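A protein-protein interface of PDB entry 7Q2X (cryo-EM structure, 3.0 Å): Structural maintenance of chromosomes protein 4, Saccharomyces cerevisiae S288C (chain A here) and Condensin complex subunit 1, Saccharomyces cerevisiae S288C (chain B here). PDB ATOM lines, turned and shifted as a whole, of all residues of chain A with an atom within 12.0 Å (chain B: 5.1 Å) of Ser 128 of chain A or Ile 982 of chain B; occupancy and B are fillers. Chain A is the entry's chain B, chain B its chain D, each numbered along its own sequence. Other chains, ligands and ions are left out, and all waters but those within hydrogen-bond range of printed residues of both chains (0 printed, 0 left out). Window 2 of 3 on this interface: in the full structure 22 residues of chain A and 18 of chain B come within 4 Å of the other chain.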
ATOM      1  N   GLN A 126      20.805  11.625  -4.586  1.00  0.00           N
ATOM      2  CA  GLN A 126      19.898  11.501  -5.722  1.00  0.00           C
ATOM      3  C   GLN A 126      19.292  12.852  -6.086  1.00  0.00           C
ATOM      4  O   GLN A 126      19.331  13.268  -7.244  1.00  0.00           O
ATOM      5  CB  GLN A 126      18.791  10.491  -5.414  1.00  0.00           C
ATOM      6  CG  GLN A 126      17.685  10.445  -6.457  1.00  0.00           C
ATOM      7  CD  GLN A 126      18.213  10.194  -7.856  1.00  0.00           C
ATOM      8  OE1 GLN A 126      18.045  11.021  -8.752  1.00  0.00           O
ATOM      9  NE2 GLN A 126      18.856   9.048  -8.048  1.00  0.00           N
ATOM     10  N   LEU A 127      18.732  13.533  -5.090  1.00  0.00           N
ATOM     11  CA  LEU A 127      18.113  14.840  -5.269  1.00  0.00           C
ATOM     12  C   LEU A 127      18.965  15.886  -4.564  1.00  0.00           C
ATOM     13  O   LEU A 127      19.257  15.752  -3.371  1.00  0.00           O
ATOM     14  CB  LEU A 127      16.685  14.850  -4.722  1.00  0.00           C
ATOM     15  CG  LEU A 127      15.659  14.001  -5.473  1.00  0.00           C
ATOM     16  CD1 LEU A 127      14.362  13.904  -4.682  1.00  0.00           C
ATOM     17  CD2 LEU A 127      15.403  14.568  -6.859  1.00  0.00           C
ATOM     18  N   SER A 128      19.363  16.918  -5.301  1.00  0.00           N
ATOM     19  CA  SER A 128      20.176  17.973  -4.717  1.00  0.00           C
ATOM     20  C   SER A 128      19.343  18.800  -3.740  1.00  0.00           C
ATOM     21  O   SER A 128      18.151  19.023  -3.973  1.00  0.00           O
ATOM     22  CB  SER A 128      20.751  18.874  -5.809  1.00  0.00           C
ATOM     23  OG  SER A 128      19.721  19.587  -6.468  1.00  0.00           O
ATOM     24  N   PRO A 129      19.936  19.259  -2.638  1.00  0.00           N
ATOM     25  CA  PRO A 129      19.175  20.065  -1.675  1.00  0.00           C
ATOM     26  C   PRO A 129      18.750  21.398  -2.274  1.00  0.00           C
ATOM     27  O   PRO A 129      19.459  21.991  -3.089  1.00  0.00           O
ATOM     28  CB  PRO A 129      20.159  20.256  -0.515  1.00  0.00           C
ATOM     29  CG  PRO A 129      21.508  20.066  -1.127  1.00  0.00           C
ATOM     30  CD  PRO A 129      21.327  19.042  -2.206  1.00  0.00           C
ATOM     31  N   VAL A 130      17.575  21.866  -1.856  1.00  0.00           N
ATOM     32  CA  VAL A 130      17.030  23.147  -2.287  1.00  0.00           C
ATOM     33  C   VAL A 130      16.559  23.911  -1.058  1.00  0.00           C
ATOM     34  O   VAL A 130      16.225  23.309  -0.031  1.00  0.00           O
ATOM     35  CB  VAL A 130      15.874  22.972  -3.294  1.00  0.00           C
ATOM     36  CG1 VAL A 130      16.382  22.362  -4.592  1.00  0.00           C
ATOM     37  CG2 VAL A 130      14.769  22.116  -2.693  1.00  0.00           C
ATOM     38  N   LYS A 131      16.537  25.236  -1.162  1.00  0.00           N
ATOM     39  CA  LYS A 131      16.089  26.096  -0.074  1.00  0.00           C
ATOM     40  C   LYS A 131      14.600  26.376  -0.242  1.00  0.00           C
ATOM     41  O   LYS A 131      14.164  26.825  -1.307  1.00  0.00           O
ATOM     42  CB  LYS A 131      16.887  27.398  -0.051  1.00  0.00           C
ATOM     43  CG  LYS A 131      18.370  27.218  -0.332  1.00  0.00           C
ATOM     44  CD  LYS A 131      19.136  28.512  -0.113  1.00  0.00           C
ATOM     45  CE  LYS A 131      20.579  28.238   0.276  1.00  0.00           C
ATOM     46  NZ  LYS A 131      21.494  29.314  -0.197  1.00  0.00           N
ATOM     47  N   ASN A 132      13.825  26.113   0.809  1.00  0.00           N
ATOM     48  CA  ASN A 132      12.378  26.287   0.776  1.00  0.00           C
ATOM     49  C   ASN A 132      11.913  27.565   1.459  1.00  0.00           C
ATOM     50  O   ASN A 132      10.982  28.215   0.974  1.00  0.00           O
ATOM     51  CB  ASN A 132      11.688  25.083   1.425  1.00  0.00           C
ATOM     52  CG  ASN A 132      10.309  24.822   0.851  1.00  0.00           C
ATOM     53  OD1 ASN A 132       9.577  25.751   0.512  1.00  0.00           O
ATOM     54  ND2 ASN A 132       9.949  23.548   0.738  1.00  0.00           N
ATOM     55  N   GLU A 136      11.338  25.282   6.734  1.00  0.00           N
ATOM     56  CA  GLU A 136      12.274  25.602   7.807  1.00  0.00           C
ATOM     57  C   GLU A 136      11.603  26.427   8.898  1.00  0.00           C
ATOM     58  O   GLU A 136      11.845  26.207  10.091  1.00  0.00           O
ATOM     59  CB  GLU A 136      13.485  26.343   7.242  1.00  0.00           C
ATOM     60  CG  GLU A 136      14.378  25.489   6.359  1.00  0.00           C
ATOM     61  CD  GLU A 136      15.486  26.290   5.704  1.00  0.00           C
ATOM     62  OE1 GLU A 136      16.187  27.035   6.421  1.00  0.00           O
ATOM     63  OE2 GLU A 136      15.657  26.173   4.472  1.00  0.00           O
ATOM     64  N   LEU B 978      10.291  21.228  -8.199  1.00  0.00           N
ATOM     65  CA  LEU B 978      11.525  21.994  -8.369  1.00  0.00           C
ATOM     66  C   LEU B 978      12.783  21.163  -8.156  1.00  0.00           C
ATOM     67  O   LEU B 978      13.716  21.291  -8.968  1.00  0.00           O
ATOM     68  CB  LEU B 978      11.497  23.220  -7.449  1.00  0.00           C
ATOM     69  CG  LEU B 978      12.627  24.230  -7.648  1.00  0.00           C
ATOM     70  CD1 LEU B 978      12.548  24.853  -9.034  1.00  0.00           C
ATOM     71  CD2 LEU B 978      12.583  25.305  -6.573  1.00  0.00           C
ATOM     72  N   PRO B 979      12.902  20.329  -7.114  1.00  0.00           N
ATOM     73  CA  PRO B 979      14.128  19.524  -6.982  1.00  0.00           C
ATOM     74  C   PRO B 979      14.394  18.620  -8.174  1.00  0.00           C
ATOM     75  O   PRO B 979      15.561  18.424  -8.533  1.00  0.00           O
ATOM     76  CB  PRO B 979      13.881  18.715  -5.702  1.00  0.00           C
ATOM     77  CG  PRO B 979      12.933  19.538  -4.922  1.00  0.00           C
ATOM     78  CD  PRO B 979      12.029  20.171  -5.935  1.00  0.00           C
ATOM     79  N   LEU B 980      13.351  18.062  -8.795  1.00  0.00           N
ATOM     80  CA  LEU B 980      13.554  17.230  -9.978  1.00  0.00           C
ATOM     81  C   LEU B 980      14.159  18.033 -11.122  1.00  0.00           C
ATOM     82  O   LEU B 980      15.114  17.588 -11.773  1.00  0.00           O
ATOM     83  CB  LEU B 980      12.229  16.600 -10.408  1.00  0.00           C
ATOM     84  CG  LEU B 980      12.292  15.559 -11.527  1.00  0.00           C
ATOM     85  CD1 LEU B 980      13.376  14.530 -11.248  1.00  0.00           C
ATOM     86  CD2 LEU B 980      10.941  14.885 -11.704  1.00  0.00           C
ATOM     87  N   LEU B 981      13.620  19.227 -11.378  1.00  0.00           N
ATOM     88  CA  LEU B 981      14.190  20.080 -12.411  1.00  0.00           C
ATOM     89  C   LEU B 981      15.619  20.477 -12.073  1.00  0.00           C
ATOM     90  O   LEU B 981      16.474  20.519 -12.963  1.00  0.00           O
ATOM     91  CB  LEU B 981      13.321  21.323 -12.608  1.00  0.00           C
ATOM     92  CG  LEU B 981      13.497  22.065 -13.933  1.00  0.00           C
ATOM     93  CD1 LEU B 981      13.282  21.122 -15.106  1.00  0.00           C
ATOM     94  CD2 LEU B 981      12.547  23.250 -14.015  1.00  0.00           C
ATOM     95  N   ILE B 982      15.899  20.751 -10.797  1.00  0.00           N
ATOM     96  CA  ILE B 982      17.248  21.142 -10.398  1.00  0.00           C
ATOM     97  C   ILE B 982      18.235  20.004 -10.630  1.00  0.00           C
ATOM     98  O   ILE B 982      19.342  20.222 -11.134  1.00  0.00           O
ATOM     99  CB  ILE B 982      17.260  21.616  -8.932  1.00  0.00           C
ATOM    100  CG1 ILE B 982      16.427  22.888  -8.772  1.00  0.00           C
ATOM    101  CG2 ILE B 982      18.683  21.860  -8.464  1.00  0.00           C
ATOM    102  CD1 ILE B 982      16.784  23.979  -9.758  1.00  0.00           C
ATOM    103  N   THR B 983      17.859  18.772 -10.268  1.00  0.00           N
ATOM    104  CA  THR B 983      18.801  17.665 -10.414  1.00  0.00           C
ATOM    105  C   THR B 983      18.963  17.266 -11.876  1.00  0.00           C
ATOM    106  O   THR B 983      20.024  16.773 -12.276  1.00  0.00           O
ATOM    107  CB  THR B 983      18.378  16.458  -9.572  1.00  0.00           C
ATOM    108  OG1 THR B 983      19.258  15.360  -9.843  1.00  0.00           O
ATOM    109  CG2 THR B 983      16.971  16.022  -9.906  1.00  0.00           C
ATOM    110  N   VAL B 984      17.922  17.462 -12.692  1.00  0.00           N
ATOM    111  CA  VAL B 984      18.077  17.253 -14.130  1.00  0.00           C
ATOM    112  C   VAL B 984      18.998  18.313 -14.723  1.00  0.00           C
ATOM    113  O   VAL B 984      19.842  18.021 -15.579  1.00  0.00           O
ATOM    114  CB  VAL B 984      16.700  17.236 -14.820  1.00  0.00           C
ATOM    115  CG1 VAL B 984      16.856  17.268 -16.332  1.00  0.00           C
ATOM    116  CG2 VAL B 984      15.929  15.999 -14.402  1.00  0.00           C
ATOM    117  N   MET B 985      18.855  19.558 -14.267  1.00  0.00           N
ATOM    118  CA  MET B 985      19.732  20.637 -14.706  1.00  0.00           C
ATOM    119  C   MET B 985      21.180  20.369 -14.306  1.00  0.00           C
ATOM    120  O   MET B 985      22.108  20.671 -15.066  1.00  0.00           O
ATOM    121  CB  MET B 985      19.229  21.951 -14.108  1.00  0.00           C
ATOM    122  CG  MET B 985      19.965  23.206 -14.509  1.00  0.00           C
ATOM    123  SD  MET B 985      19.132  24.619 -13.756  1.00  0.00           S
ATOM    124  CE  MET B 985      20.193  25.965 -14.249  1.00  0.00           C
ATOM    125  N   GLU B 986      21.389  19.807 -13.113  1.00  0.00           N
ATOM    126  CA  GLU B 986      22.738  19.487 -12.654  1.00  0.00           C
ATOM    127  C   GLU B 986      23.382  18.407 -13.514  1.00  0.00           C
ATOM    128  O   GLU B 986      24.549  18.531 -13.903  1.00  0.00           O
ATOM    129  CB  GLU B 986      22.699  19.043 -11.191  1.00  0.00           C
ATOM    130  CG  GLU B 986      22.424  20.155 -10.193  1.00  0.00           C
ATOM    131  CD  GLU B 986      23.555  21.161 -10.114  1.00  0.00           C
ATOM    132  OE1 GLU B 986      24.726  20.750 -10.252  1.00  0.00           O
ATOM    133  OE2 GLU B 986      23.273  22.362  -9.915  1.00  0.00           O
ATOM    134  N   LEU B1001      13.952  27.792 -15.271  1.00  0.00           N
ATOM    135  CA  LEU B1001      14.312  28.444 -14.016  1.00  0.00           C
ATOM    136  C   LEU B1001      14.158  29.956 -14.126  1.00  0.00           C
ATOM    137  O   LEU B1001      13.653  30.605 -13.202  1.00  0.00           O
ATOM    138  CB  LEU B1001      15.738  28.073 -13.609  1.00  0.00           C
ATOM    139  CG  LEU B1001      15.920  26.878 -12.666  1.00  0.00           C
ATOM    140  CD1 LEU B1001      15.299  27.171 -11.309  1.00  0.00           C
ATOM    141  CD2 LEU B1001      15.347  25.596 -13.251  1.00  0.00           C
ATOM    142  N   TYR B1018      21.389  28.609  -8.486  1.00  0.00           N
ATOM    143  CA  TYR B1018      21.596  27.453  -9.350  1.00  0.00           C
ATOM    144  C   TYR B1018      21.883  27.884 -10.784  1.00  0.00           C
ATOM    145  O   TYR B1018      22.738  27.297 -11.456  1.00  0.00           O
ATOM    146  CB  TYR B1018      20.377  26.534  -9.293  1.00  0.00           C
ATOM    147  CG  TYR B1018      20.411  25.549  -8.146  1.00  0.00           C
ATOM    148  CD1 TYR B1018      21.526  24.753  -7.921  1.00  0.00           C
ATOM    149  CD2 TYR B1018      19.332  25.425  -7.281  1.00  0.00           C
ATOM    150  CE1 TYR B1018      21.565  23.856  -6.872  1.00  0.00           C
ATOM    151  CE2 TYR B1018      19.362  24.530  -6.227  1.00  0.00           C
ATOM    152  CZ  TYR B1018      20.480  23.748  -6.027  1.00  0.00           C
ATOM    153  OH  TYR B1018      20.514  22.856  -4.981  1.00  0.00           O
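The backbone carbonyl oxygen (O) of Gln 126 of chain A lies within hydrogen-bond range of the side-chain hydroxyl (OG1) of Thr 983 of chain B (3.3 Å). OH of Tyr 1018 of chain B lies close to O of Pro 129 of chain A (2.3 Å).
Leu 127 of chain A touches Thr 983 of chain B (CD2 to CG2, 3.7 Å). OG of Ser 128 of chain A touches CG2 of Ile 982 of chain B (3.2 Å). Tyr 1018 of chain B touches Ser 128 of chain A. Pro 979 of chain B touches Val 130 of chain A (CG to CG2, 3.9 Å).
Of the printed residues of chain B, Gln 126 of chain A touches Thr 983 (3.3 Å). Of the printed residues of chain B, Leu 127 of chain A touches Thr 983. Printed residues of chain B within 4 Å of Pro 129 of chain A: Tyr 1018 (2.3 Å). Of the printed residues of chain B, Val 130 of chain A touches Pro 979. No residue of chain A comes within 4 Å of Leu 980 of chain B. No residue of chain A comes within 4 Å of Leu 981 of chain B. Ile 982 of chain B touches just one residue of chain A: Ser 128. Of the printed residues of chain A, Thr 983 of chain B touches Gln 126 and Leu 127. No residue of chain A comes within 4 Å of Val 984 of chain B. No residue of chain A comes within 4 Å of Met 985 of chain B. No residue of chain A comes within 4 Å of Glu 986 of chain B. Tyr 1018 of chain B touches just these residues of chain A: Ser 128 (3.7 Å) and Pro 129 (2.3 Å). The nearest residue of chain B that does not touch Ser 128 of chain A is Thr 983 of chain B (4.3 Å).
Of the 8 printed residues of chain A, 5 touch a printed residue of chain B. Hydrophobic or aromatic side chains of chain A that line the printed part of chain B: Leu 127 and Val 130. Of the 11 printed residues of chain B, 4 touch a printed residue of chain A. Hydrophobic or aromatic side chains of chain B that line the printed part of chain A: Pro 979, Ile 982 and Tyr 1018. Among the printed residues, no Asp or Glu carboxylate lies within 4 Å of a Lys or Arg side-chain nitrogen of the other chain.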
